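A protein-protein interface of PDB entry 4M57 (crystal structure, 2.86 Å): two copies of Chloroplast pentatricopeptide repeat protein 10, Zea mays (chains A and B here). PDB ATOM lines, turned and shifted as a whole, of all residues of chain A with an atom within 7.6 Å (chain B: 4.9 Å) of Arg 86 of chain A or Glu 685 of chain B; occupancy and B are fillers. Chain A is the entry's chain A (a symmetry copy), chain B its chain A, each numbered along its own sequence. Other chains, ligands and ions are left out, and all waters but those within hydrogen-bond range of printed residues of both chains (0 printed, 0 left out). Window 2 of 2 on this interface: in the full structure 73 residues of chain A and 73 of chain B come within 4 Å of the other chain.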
ATOM      1  N   SER A  10     -32.368 -15.270   7.048  1.00  0.00           N
ATOM      2  CA  SER A  10     -32.742 -16.625   6.667  1.00  0.00           C
ATOM      3  C   SER A  10     -32.353 -17.589   7.751  1.00  0.00           C
ATOM      4  O   SER A  10     -32.440 -18.797   7.596  1.00  0.00           O
ATOM      5  CB  SER A  10     -32.004 -17.029   5.402  1.00  0.00           C
ATOM      6  OG  SER A  10     -30.823 -17.734   5.726  1.00  0.00           O
ATOM      7  N   LYS A  52     -22.930 -11.713  11.911  1.00  0.00           N
ATOM      8  CA  LYS A  52     -22.998 -12.493  10.674  1.00  0.00           C
ATOM      9  C   LYS A  52     -24.016 -11.917   9.692  1.00  0.00           C
ATOM     10  O   LYS A  52     -23.730 -11.728   8.499  1.00  0.00           O
ATOM     11  CB  LYS A  52     -23.310 -13.964  10.960  1.00  0.00           C
ATOM     12  CG  LYS A  52     -23.369 -14.818   9.707  1.00  0.00           C
ATOM     13  CD  LYS A  52     -23.252 -16.292   9.994  1.00  0.00           C
ATOM     14  CE  LYS A  52     -24.542 -16.894  10.542  1.00  0.00           C
ATOM     15  NZ  LYS A  52     -24.438 -18.387  10.763  1.00  0.00           N
ATOM     16  N   GLU A  55     -22.790  -8.875   8.090  1.00  0.00           N
ATOM     17  CA  GLU A  55     -21.793  -9.180   7.070  1.00  0.00           C
ATOM     18  C   GLU A  55     -22.453  -9.612   5.759  1.00  0.00           C
ATOM     19  O   GLU A  55     -22.041  -9.195   4.677  1.00  0.00           O
ATOM     20  CB  GLU A  55     -20.839 -10.269   7.562  1.00  0.00           C
ATOM     21  CG  GLU A  55     -19.698 -10.575   6.605  1.00  0.00           C
ATOM     22  CD  GLU A  55     -19.689  -9.657   5.399  1.00  0.00           C
ATOM     23  OE1 GLU A  55     -19.593 -10.167   4.263  1.00  0.00           O
ATOM     24  OE2 GLU A  55     -19.777  -8.426   5.587  1.00  0.00           O
ATOM     25  N   LEU A  56     -23.479 -10.450   5.869  1.00  0.00           N
ATOM     26  CA  LEU A  56     -24.208 -10.952   4.717  1.00  0.00           C
ATOM     27  C   LEU A  56     -25.111  -9.891   4.080  1.00  0.00           C
ATOM     28  O   LEU A  56     -25.644 -10.099   2.994  1.00  0.00           O
ATOM     29  CB  LEU A  56     -25.028 -12.193   5.099  1.00  0.00           C
ATOM     30  CG  LEU A  56     -24.313 -13.530   5.297  1.00  0.00           C
ATOM     31  CD1 LEU A  56     -25.203 -14.518   6.011  1.00  0.00           C
ATOM     32  CD2 LEU A  56     -23.886 -14.087   3.977  1.00  0.00           C
ATOM     33  N   ALA A  80     -17.684 -13.937  18.223  1.00  0.00           N
ATOM     34  CA  ALA A  80     -18.020 -12.623  17.668  1.00  0.00           C
ATOM     35  C   ALA A  80     -16.815 -11.942  16.996  1.00  0.00           C
ATOM     36  O   ALA A  80     -16.897 -11.417  15.860  1.00  0.00           O
ATOM     37  CB  ALA A  80     -18.586 -11.732  18.761  1.00  0.00           C
ATOM     38  N   LEU A  81     -15.698 -11.950  17.720  1.00  0.00           N
ATOM     39  CA  LEU A  81     -14.449 -11.444  17.188  1.00  0.00           C
ATOM     40  C   LEU A  81     -14.032 -12.209  15.949  1.00  0.00           C
ATOM     41  O   LEU A  81     -13.566 -11.620  14.990  1.00  0.00           O
ATOM     42  CB  LEU A  81     -13.331 -11.532  18.213  1.00  0.00           C
ATOM     43  CG  LEU A  81     -12.081 -10.825  17.700  1.00  0.00           C
ATOM     44  CD1 LEU A  81     -12.082  -9.399  18.202  1.00  0.00           C
ATOM     45  CD2 LEU A  81     -10.847 -11.573  18.144  1.00  0.00           C
ATOM     46  N   GLU A  82     -14.187 -13.522  15.954  1.00  0.00           N
ATOM     47  CA  GLU A  82     -13.773 -14.244  14.773  1.00  0.00           C
ATOM     48  C   GLU A  82     -14.722 -14.025  13.619  1.00  0.00           C
ATOM     49  O   GLU A  82     -14.307 -14.069  12.471  1.00  0.00           O
ATOM     50  CB  GLU A  82     -13.551 -15.717  15.061  1.00  0.00           C
ATOM     51  CG  GLU A  82     -12.248 -15.938  15.779  1.00  0.00           C
ATOM     52  CD  GLU A  82     -11.798 -17.374  15.748  1.00  0.00           C
ATOM     53  OE1 GLU A  82     -12.501 -18.208  15.123  1.00  0.00           O
ATOM     54  OE2 GLU A  82     -10.738 -17.662  16.350  1.00  0.00           O
ATOM     55  N   MET A  83     -15.994 -13.788  13.920  1.00  0.00           N
ATOM     56  CA  MET A  83     -16.953 -13.525  12.861  1.00  0.00           C
ATOM     57  C   MET A  83     -16.575 -12.231  12.166  1.00  0.00           C
ATOM     58  O   MET A  83     -16.565 -12.167  10.946  1.00  0.00           O
ATOM     59  CB  MET A  83     -18.390 -13.442  13.387  1.00  0.00           C
ATOM     60  CG  MET A  83     -19.428 -13.325  12.267  1.00  0.00           C
ATOM     61  SD  MET A  83     -19.595 -14.848  11.331  1.00  0.00           S
ATOM     62  CE  MET A  83     -19.752 -14.213   9.681  1.00  0.00           C
ATOM     63  N   VAL A  84     -16.242 -11.201  12.939  1.00  0.00           N
ATOM     64  CA  VAL A  84     -15.881  -9.926  12.329  1.00  0.00           C
ATOM     65  C   VAL A  84     -14.503  -9.958  11.650  1.00  0.00           C
ATOM     66  O   VAL A  84     -14.306  -9.335  10.612  1.00  0.00           O
ATOM     67  CB  VAL A  84     -15.937  -8.768  13.336  1.00  0.00           C
ATOM     68  CG1 VAL A  84     -15.639  -7.450  12.639  1.00  0.00           C
ATOM     69  CG2 VAL A  84     -17.298  -8.726  14.025  1.00  0.00           C
ATOM     70  N   VAL A  85     -13.545 -10.673  12.238  1.00  0.00           N
ATOM     71  CA  VAL A  85     -12.224 -10.786  11.631  1.00  0.00           C
ATOM     72  C   VAL A  85     -12.324 -11.514  10.293  1.00  0.00           C
ATOM     73  O   VAL A  85     -11.718 -11.093   9.291  1.00  0.00           O
ATOM     74  CB  VAL A  85     -11.207 -11.474  12.563  1.00  0.00           C
ATOM     75  CG1 VAL A  85     -10.056 -12.055  11.764  1.00  0.00           C
ATOM     76  CG2 VAL A  85     -10.698 -10.493  13.620  1.00  0.00           C
ATOM     77  N   ARG A  86     -13.103 -12.591  10.271  1.00  0.00           N
ATOM     78  CA  ARG A  86     -13.353 -13.301   9.026  1.00  0.00           C
ATOM     79  C   ARG A  86     -14.084 -12.395   8.037  1.00  0.00           C
ATOM     80  O   ARG A  86     -13.784 -12.410   6.836  1.00  0.00           O
ATOM     81  CB  ARG A  86     -14.139 -14.593   9.264  1.00  0.00           C
ATOM     82  CG  ARG A  86     -14.853 -15.125   8.027  1.00  0.00           C
ATOM     83  CD  ARG A  86     -15.350 -16.565   8.171  1.00  0.00           C
ATOM     84  NE  ARG A  86     -15.989 -17.023   6.937  1.00  0.00           N
ATOM     85  CZ  ARG A  86     -16.427 -18.257   6.716  1.00  0.00           C
ATOM     86  NH1 ARG A  86     -16.300 -19.189   7.642  1.00  0.00           N
ATOM     87  NH2 ARG A  86     -16.993 -18.562   5.559  1.00  0.00           N
ATOM     88  N   ALA A  87     -15.019 -11.592   8.541  1.00  0.00           N
ATOM     89  CA  ALA A  87     -15.800 -10.704   7.677  1.00  0.00           C
ATOM     90  C   ALA A  87     -14.930  -9.650   7.003  1.00  0.00           C
ATOM     91  O   ALA A  87     -14.907  -9.558   5.786  1.00  0.00           O
ATOM     92  CB  ALA A  87     -16.946 -10.042   8.448  1.00  0.00           C
ATOM     93  N   LEU A  88     -14.231  -8.848   7.798  1.00  0.00           N
ATOM     94  CA  LEU A  88     -13.355  -7.807   7.265  1.00  0.00           C
ATOM     95  C   LEU A  88     -12.263  -8.410   6.387  1.00  0.00           C
ATOM     96  O   LEU A  88     -11.823  -7.791   5.425  1.00  0.00           O
ATOM     97  CB  LEU A  88     -12.724  -6.995   8.390  1.00  0.00           C
ATOM     98  CG  LEU A  88     -13.612  -6.352   9.446  1.00  0.00           C
ATOM     99  CD1 LEU A  88     -12.808  -5.458  10.376  1.00  0.00           C
ATOM    100  CD2 LEU A  88     -14.690  -5.566   8.762  1.00  0.00           C
ATOM    101  N   GLY A  89     -11.825  -9.616   6.734  1.00  0.00           N
ATOM    102  CA  GLY A  89     -10.882 -10.342   5.909  1.00  0.00           C
ATOM    103  C   GLY A  89     -11.420 -10.583   4.519  1.00  0.00           C
ATOM    104  O   GLY A  89     -10.796 -10.208   3.537  1.00  0.00           O
ATOM    105  N   ARG A  90     -12.589 -11.208   4.435  1.00  0.00           N
ATOM    106  CA  ARG A  90     -13.242 -11.482   3.151  1.00  0.00           C
ATOM    107  C   ARG A  90     -13.611 -10.183   2.422  1.00  0.00           C
ATOM    108  O   ARG A  90     -13.623 -10.116   1.194  1.00  0.00           O
ATOM    109  CB  ARG A  90     -14.454 -12.413   3.367  1.00  0.00           C
ATOM    110  CG  ARG A  90     -15.711 -12.158   2.514  1.00  0.00           C
ATOM    111  CD  ARG A  90     -16.951 -12.871   3.113  1.00  0.00           C
ATOM    112  NE  ARG A  90     -18.158 -12.725   2.289  1.00  0.00           N
ATOM    113  CZ  ARG A  90     -19.391 -13.053   2.684  1.00  0.00           C
ATOM    114  NH1 ARG A  90     -19.605 -13.551   3.909  1.00  0.00           N
ATOM    115  NH2 ARG A  90     -20.416 -12.881   1.851  1.00  0.00           N
ATOM    116  N   GLU A  91     -13.866  -9.144   3.200  1.00  0.00           N
ATOM    117  CA  GLU A  91     -14.223  -7.856   2.657  1.00  0.00           C
ATOM    118  C   GLU A  91     -12.984  -7.064   2.206  1.00  0.00           C
ATOM    119  O   GLU A  91     -13.108  -5.990   1.609  1.00  0.00           O
ATOM    120  CB  GLU A  91     -15.033  -7.080   3.694  1.00  0.00           C
ATOM    121  CG  GLU A  91     -16.111  -6.173   3.104  1.00  0.00           C
ATOM    122  CD  GLU A  91     -17.362  -6.925   2.646  1.00  0.00           C
ATOM    123  OE1 GLU A  91     -17.690  -6.824   1.446  1.00  0.00           O
ATOM    124  OE2 GLU A  91     -18.027  -7.592   3.480  1.00  0.00           O
ATOM    125  N   GLY A  92     -11.796  -7.605   2.485  1.00  0.00           N
ATOM    126  CA  GLY A  92     -10.534  -6.969   2.129  1.00  0.00           C
ATOM    127  C   GLY A  92     -10.161  -5.736   2.943  1.00  0.00           C
ATOM    128  O   GLY A  92      -9.402  -4.888   2.494  1.00  0.00           O
ATOM    129  N   VAL A  97      -9.113  -4.212  10.308  1.00  0.00           N
ATOM    130  CA  VAL A  97      -8.807  -5.408  11.088  1.00  0.00           C
ATOM    131  C   VAL A  97      -7.628  -5.168  12.017  1.00  0.00           C
ATOM    132  O   VAL A  97      -7.711  -5.428  13.223  1.00  0.00           O
ATOM    133  CB  VAL A  97      -8.457  -6.612  10.226  1.00  0.00           C
ATOM    134  CG1 VAL A  97      -8.191  -7.805  11.102  1.00  0.00           C
ATOM    135  CG2 VAL A  97      -9.581  -6.944   9.361  1.00  0.00           C
ATOM    136  N   ASP A 113      -9.778 -20.374  15.803  1.00  0.00           N
ATOM    137  CA  ASP A 113      -9.803 -21.189  14.605  1.00  0.00           C
ATOM    138  C   ASP A 113      -8.960 -20.519  13.519  1.00  0.00           C
ATOM    139  O   ASP A 113      -9.381 -19.509  12.961  1.00  0.00           O
ATOM    140  CB  ASP A 113     -11.236 -21.369  14.118  1.00  0.00           C
ATOM    141  CG  ASP A 113     -11.360 -22.483  13.105  1.00  0.00           C
ATOM    142  OD1 ASP A 113     -10.365 -23.226  12.923  1.00  0.00           O
ATOM    143  OD2 ASP A 113     -12.448 -22.624  12.504  1.00  0.00           O
ATOM    144  N   ARG A 115      -8.552 -20.780  10.579  1.00  0.00           N
ATOM    145  CA  ARG A 115      -9.146 -20.558   9.276  1.00  0.00           C
ATOM    146  C   ARG A 115      -9.756 -19.167   9.121  1.00  0.00           C
ATOM    147  O   ARG A 115      -9.881 -18.673   8.005  1.00  0.00           O
ATOM    148  CB  ARG A 115     -10.205 -21.604   8.981  1.00  0.00           C
ATOM    149  CG  ARG A 115      -9.872 -22.989   9.408  1.00  0.00           C
ATOM    150  CD  ARG A 115     -11.169 -23.638   9.853  1.00  0.00           C
ATOM    151  NE  ARG A 115     -11.267 -25.036   9.464  1.00  0.00           N
ATOM    152  CZ  ARG A 115     -12.408 -25.625   9.128  1.00  0.00           C
ATOM    153  NH1 ARG A 115     -13.548 -24.931   9.142  1.00  0.00           N
ATOM    154  NH2 ARG A 115     -12.414 -26.908   8.776  1.00  0.00           N
ATOM    155  N   ALA A 116     -10.127 -18.548  10.239  1.00  0.00           N
ATOM    156  CA  ALA A 116     -10.755 -17.226  10.253  1.00  0.00           C
ATOM    157  C   ALA A 116      -9.805 -16.120   9.866  1.00  0.00           C
ATOM    158  O   ALA A 116     -10.244 -14.989   9.635  1.00  0.00           O
ATOM    159  CB  ALA A 116     -11.300 -16.926  11.625  1.00  0.00           C
ATOM    160  N   TYR A 117      -8.509 -16.428   9.811  1.00  0.00           N
ATOM    161  CA  TYR A 117      -7.497 -15.384   9.703  1.00  0.00           C
ATOM    162  C   TYR A 117      -6.803 -15.312   8.343  1.00  0.00           C
ATOM    163  O   TYR A 117      -6.243 -14.269   7.960  1.00  0.00           O
ATOM    164  CB  TYR A 117      -6.495 -15.528  10.840  1.00  0.00           C
ATOM    165  CG  TYR A 117      -7.153 -15.422  12.188  1.00  0.00           C
ATOM    166  CD1 TYR A 117      -7.404 -14.187  12.764  1.00  0.00           C
ATOM    167  CD2 TYR A 117      -7.544 -16.556  12.874  1.00  0.00           C
ATOM    168  CE1 TYR A 117      -8.009 -14.085  13.988  1.00  0.00           C
ATOM    169  CE2 TYR A 117      -8.161 -16.471  14.111  1.00  0.00           C
ATOM    170  CZ  TYR A 117      -8.397 -15.232  14.670  1.00  0.00           C
ATOM    171  OH  TYR A 117      -9.021 -15.153  15.911  1.00  0.00           O
ATOM    172  N   THR A 118      -6.889 -16.421   7.616  1.00  0.00           N
ATOM    173  CA  THR A 118      -6.287 -16.579   6.300  1.00  0.00           C
ATOM    174  C   THR A 118      -6.497 -15.369   5.391  1.00  0.00           C
ATOM    175  O   THR A 118      -5.524 -14.705   5.013  1.00  0.00           O
ATOM    176  CB  THR A 118      -6.802 -17.857   5.621  1.00  0.00           C
ATOM    177  OG1 THR A 118      -6.498 -18.986   6.451  1.00  0.00           O
ATOM    178  CG2 THR A 118      -6.162 -18.038   4.261  1.00  0.00           C
ATOM    179  N   THR A 119      -7.755 -15.072   5.071  1.00  0.00           N
ATOM    180  CA  THR A 119      -8.085 -13.922   4.222  1.00  0.00           C
ATOM    181  C   THR A 119      -7.398 -12.624   4.688  1.00  0.00           C
ATOM    182  O   THR A 119      -6.791 -11.913   3.874  1.00  0.00           O
ATOM    183  CB  THR A 119      -9.634 -13.715   4.076  1.00  0.00           C
ATOM    184  OG1 THR A 119     -10.288 -13.974   5.332  1.00  0.00           O
ATOM    185  CG2 THR A 119     -10.205 -14.652   3.023  1.00  0.00           C
ATOM    186  N   VAL A 120      -7.447 -12.340   5.991  1.00  0.00           N
ATOM    187  CA  VAL A 120      -6.814 -11.125   6.505  1.00  0.00           C
ATOM    188  C   VAL A 120      -5.320 -11.186   6.194  1.00  0.00           C
ATOM    189  O   VAL A 120      -4.749 -10.261   5.605  1.00  0.00           O
ATOM    190  CB  VAL A 120      -7.013 -10.957   8.040  1.00  0.00           C
ATOM    191  CG1 VAL A 120      -6.316  -9.711   8.525  1.00  0.00           C
ATOM    192  CG2 VAL A 120      -8.474 -10.867   8.391  1.00  0.00           C
ATOM    193  N   LEU B 678     -11.890 -23.588   4.560  1.00  0.00           N
ATOM    194  CA  LEU B 678     -12.886 -22.539   4.461  1.00  0.00           C
ATOM    195  C   LEU B 678     -13.793 -22.657   3.242  1.00  0.00           C
ATOM    196  O   LEU B 678     -14.935 -22.219   3.274  1.00  0.00           O
ATOM    197  CB  LEU B 678     -12.188 -21.188   4.424  1.00  0.00           C
ATOM    198  CG  LEU B 678     -12.840 -20.116   5.291  1.00  0.00           C
ATOM    199  CD1 LEU B 678     -13.176 -20.697   6.652  1.00  0.00           C
ATOM    200  CD2 LEU B 678     -11.920 -18.909   5.427  1.00  0.00           C
ATOM    201  N   ARG B 681     -16.275 -25.378   3.763  1.00  0.00           N
ATOM    202  CA  ARG B 681     -17.121 -24.743   4.759  1.00  0.00           C
ATOM    203  C   ARG B 681     -18.144 -23.791   4.125  1.00  0.00           C
ATOM    204  O   ARG B 681     -19.315 -23.812   4.495  1.00  0.00           O
ATOM    205  CB  ARG B 681     -16.259 -23.987   5.765  1.00  0.00           C
ATOM    206  CG  ARG B 681     -16.563 -24.325   7.189  1.00  0.00           C
ATOM    207  CD  ARG B 681     -17.655 -23.452   7.740  1.00  0.00           C
ATOM    208  NE  ARG B 681     -17.649 -23.439   9.202  1.00  0.00           N
ATOM    209  CZ  ARG B 681     -18.322 -22.568   9.947  1.00  0.00           C
ATOM    210  NH1 ARG B 681     -19.064 -21.627   9.377  1.00  0.00           N
ATOM    211  NH2 ARG B 681     -18.253 -22.637  11.267  1.00  0.00           N
ATOM    212  N   ARG B 682     -17.695 -22.987   3.165  1.00  0.00           N
ATOM    213  CA  ARG B 682     -18.498 -21.939   2.543  1.00  0.00           C
ATOM    214  C   ARG B 682     -19.623 -22.521   1.737  1.00  0.00           C
ATOM    215  O   ARG B 682     -20.767 -22.030   1.783  1.00  0.00           O
ATOM    216  CB  ARG B 682     -17.630 -21.114   1.588  1.00  0.00           C
ATOM    217  CG  ARG B 682     -17.494 -19.648   1.956  1.00  0.00           C
ATOM    218  CD  ARG B 682     -18.321 -18.741   1.056  1.00  0.00           C
ATOM    219  NE  ARG B 682     -19.755 -18.916   1.269  1.00  0.00           N
ATOM    220  CZ  ARG B 682     -20.687 -18.040   0.898  1.00  0.00           C
ATOM    221  NH1 ARG B 682     -20.354 -16.891   0.295  1.00  0.00           N
ATOM    222  NH2 ARG B 682     -21.960 -18.316   1.148  1.00  0.00           N
ATOM    223  N   VAL B 683     -19.288 -23.546   0.959  1.00  0.00           N
ATOM    224  CA  VAL B 683     -20.329 -24.263   0.230  1.00  0.00           C
ATOM    225  C   VAL B 683     -21.381 -24.759   1.216  1.00  0.00           C
ATOM    226  O   VAL B 683     -22.572 -24.488   1.057  1.00  0.00           O
ATOM    227  CB  VAL B 683     -19.777 -25.457  -0.553  1.00  0.00           C
ATOM    228  CG1 VAL B 683     -20.923 -26.201  -1.215  1.00  0.00           C
ATOM    229  CG2 VAL B 683     -18.781 -24.985  -1.593  1.00  0.00           C
ATOM    230  N   VAL B 684     -20.926 -25.463   2.251  1.00  0.00           N
ATOM    231  CA  VAL B 684     -21.833 -25.964   3.270  1.00  0.00           C
ATOM    232  C   VAL B 684     -22.715 -24.874   3.897  1.00  0.00           C
ATOM    233  O   VAL B 684     -23.900 -25.093   4.119  1.00  0.00           O
ATOM    234  CB  VAL B 684     -21.094 -26.755   4.357  1.00  0.00           C
ATOM    235  CG1 VAL B 684     -22.066 -27.233   5.400  1.00  0.00           C
ATOM    236  CG2 VAL B 684     -20.394 -27.950   3.755  1.00  0.00           C
ATOM    237  N   GLU B 685     -22.152 -23.701   4.164  1.00  0.00           N
ATOM    238  CA  GLU B 685     -22.918 -22.597   4.739  1.00  0.00           C
ATOM    239  C   GLU B 685     -24.027 -22.165   3.812  1.00  0.00           C
ATOM    240  O   GLU B 685     -25.169 -22.007   4.240  1.00  0.00           O
ATOM    241  CB  GLU B 685     -22.032 -21.390   5.030  1.00  0.00           C
ATOM    242  CG  GLU B 685     -20.984 -21.608   6.093  1.00  0.00           C
ATOM    243  CD  GLU B 685     -19.894 -20.533   6.067  1.00  0.00           C
ATOM    244  OE1 GLU B 685     -19.893 -19.682   5.131  1.00  0.00           O
ATOM    245  OE2 GLU B 685     -19.036 -20.548   6.985  1.00  0.00           O
ATOM    246  N   SER B 686     -23.700 -21.960   2.539  1.00  0.00           N
ATOM    247  CA  SER B 686     -24.742 -21.573   1.581  1.00  0.00           C
ATOM    248  C   SER B 686     -25.857 -22.630   1.440  1.00  0.00           C
ATOM    249  O   SER B 686     -27.038 -22.282   1.362  1.00  0.00           O
ATOM    250  CB  SER B 686     -24.142 -21.220   0.224  1.00  0.00           C
ATOM    251  OG  SER B 686     -24.063 -19.823   0.090  1.00  0.00           O
ATOM    252  N   TYR B 687     -25.467 -23.907   1.403  1.00  0.00           N
ATOM    253  CA  TYR B 687     -26.424 -25.000   1.448  1.00  0.00           C
ATOM    254  C   TYR B 687     -27.353 -24.884   2.678  1.00  0.00           C
ATOM    255  O   TYR B 687     -28.575 -25.029   2.574  1.00  0.00           O
ATOM    256  CB  TYR B 687     -25.685 -26.340   1.513  1.00  0.00           C
ATOM    257  CG  TYR B 687     -25.406 -27.050   0.192  1.00  0.00           C
ATOM    258  CD1 TYR B 687     -26.396 -27.228  -0.759  1.00  0.00           C
ATOM    259  CD2 TYR B 687     -24.151 -27.597  -0.070  1.00  0.00           C
ATOM    260  CE1 TYR B 687     -26.131 -27.895  -1.956  1.00  0.00           C
ATOM    261  CE2 TYR B 687     -23.877 -28.259  -1.256  1.00  0.00           C
ATOM    262  CZ  TYR B 687     -24.866 -28.406  -2.198  1.00  0.00           C
ATOM    263  OH  TYR B 687     -24.591 -29.075  -3.375  1.00  0.00           O
ATOM    264  N   CYS B 688     -26.764 -24.617   3.840  1.00  0.00           N
ATOM    265  CA  CYS B 688     -27.503 -24.600   5.108  1.00  0.00           C
ATOM    266  C   CYS B 688     -28.426 -23.409   5.257  1.00  0.00           C
ATOM    267  O   CYS B 688     -29.419 -23.488   5.979  1.00  0.00           O
ATOM    268  CB  CYS B 688     -26.557 -24.653   6.312  1.00  0.00           C
ATOM    269  SG  CYS B 688     -25.786 -26.262   6.597  1.00  0.00           S
ATOM    270  N   ARG B 689     -28.101 -22.299   4.598  1.00  0.00           N
ATOM    271  CA  ARG B 689     -29.019 -21.166   4.644  1.00  0.00           C
ATOM    272  C   ARG B 689     -30.157 -21.352   3.649  1.00  0.00           C
ATOM    273  O   ARG B 689     -31.282 -20.907   3.890  1.00  0.00           O
ATOM    274  CB  ARG B 689     -28.303 -19.825   4.471  1.00  0.00           C
ATOM    275  CG  ARG B 689     -27.556 -19.369   5.738  1.00  0.00           C
ATOM    276  CD  ARG B 689     -26.840 -18.011   5.568  1.00  0.00           C
ATOM    277  NE  ARG B 689     -25.881 -17.979   4.457  1.00  0.00           N
ATOM    278  CZ  ARG B 689     -24.560 -18.102   4.591  1.00  0.00           C
ATOM    279  NH1 ARG B 689     -24.022 -18.261   5.799  1.00  0.00           N
ATOM    280  NH2 ARG B 689     -23.770 -18.061   3.518  1.00  0.00           N
ATOM    281  N   TYR B 718     -21.277 -29.672  11.884  1.00  0.00           N
ATOM    282  CA  TYR B 718     -21.828 -28.353  11.706  1.00  0.00           C
ATOM    283  C   TYR B 718     -23.227 -28.497  11.178  1.00  0.00           C
ATOM    284  O   TYR B 718     -24.151 -28.032  11.810  1.00  0.00           O
ATOM    285  CB  TYR B 718     -20.980 -27.556  10.723  1.00  0.00           C
ATOM    286  CG  TYR B 718     -21.512 -26.171  10.420  1.00  0.00           C
ATOM    287  CD1 TYR B 718     -21.373 -25.140  11.338  1.00  0.00           C
ATOM    288  CD2 TYR B 718     -22.145 -25.893   9.210  1.00  0.00           C
ATOM    289  CE1 TYR B 718     -21.846 -23.865  11.062  1.00  0.00           C
ATOM    290  CE2 TYR B 718     -22.623 -24.623   8.925  1.00  0.00           C
ATOM    291  CZ  TYR B 718     -22.471 -23.610   9.857  1.00  0.00           C
ATOM    292  OH  TYR B 718     -22.942 -22.343   9.592  1.00  0.00           O
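Ser 10 of chain A touches Arg 689 of chain B.
NE of Arg 689 of chain B touches CD1 of Leu 56 of chain A, 3.9 Å away.
Leu 678 of chain B touches Arg 86 of chain A (CD1 to NH1, 3.6 Å).
Arg 682 of chain B touches Arg 86 of chain A.
Leu 678 of chain B touches Arg 115 of chain A (CD2 to O, 3.3 Å).
CG of Arg 681 of chain B touches NH1 of Arg 115 of chain A, 3.6 Å away.
The guanidinium group of Arg 86 of chain A lies within salt-bridge range of the side-chain carboxylate of Glu 685 of chain B (3.1 Å).
No position is printed for both chains.
Of the 7 pairs that touch across the chains among the printed residues, none has its exchanged pair printed and touching as well.
Of the printed residues of chain B, Leu 56 of chain A touches Arg 689.
Of chain B, only Leu 678, Arg 682 and Glu 685 come within 4 Å of Arg 86 of chain A.
Of the printed residues of chain B, Arg 115 of chain A touches Leu 678 (3.3 Å) and Arg 681 (3.6 Å).
Val 120 of chain A touches none of the printed residues of chain B.
Of the printed residues of chain A, Arg 681 of chain B touches Arg 115 (3.6 Å).
Of the printed residues of chain A, Arg 682 of chain B touches Arg 86.
Val 683 of chain B touches none of the printed residues of chain A.
Of the printed residues of chain A, Arg 689 of chain B touches Ser 10 (3.5 Å) and Leu 56 (3.9 Å).
The nearest printed residue of chain A that does not touch Arg 689 of chain B is Lys 52 of chain A (4.7 Å).
The guanidinium group (NE) of Arg 682 of chain B lies within salt-bridge range of the side-chain carboxylate (OE1) of Glu 685 of chain B (3.9 Å).
NH1 of Arg 681 of chain B lies within salt-bridge range of OE2 of Glu 685 of chain B.
The guanidinium group (NH2) of Arg 682 of chain B sits at hydrogen-bond distance from the side-chain hydroxyl (OG) of Ser 686 of chain B (2.8 Å).
Hydrophobic or aromatic side chains of chain A that line the printed part of chain B: Leu 56.
Along chain A the printed residues that touch a printed residue of chain B span positions 10 to 115.
Hydrophobic or aromatic side chains of chain B that line the printed part of chain A: Leu 678.
Among the printed residues, 7 pairs touch across the chains.
Among the printed residues, Asp or Glu carboxylates within 4 Å of a Lys or Arg side-chain nitrogen of the other chain: Arg 86 of chain A with Glu 685 of chain B (3.1 Å).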
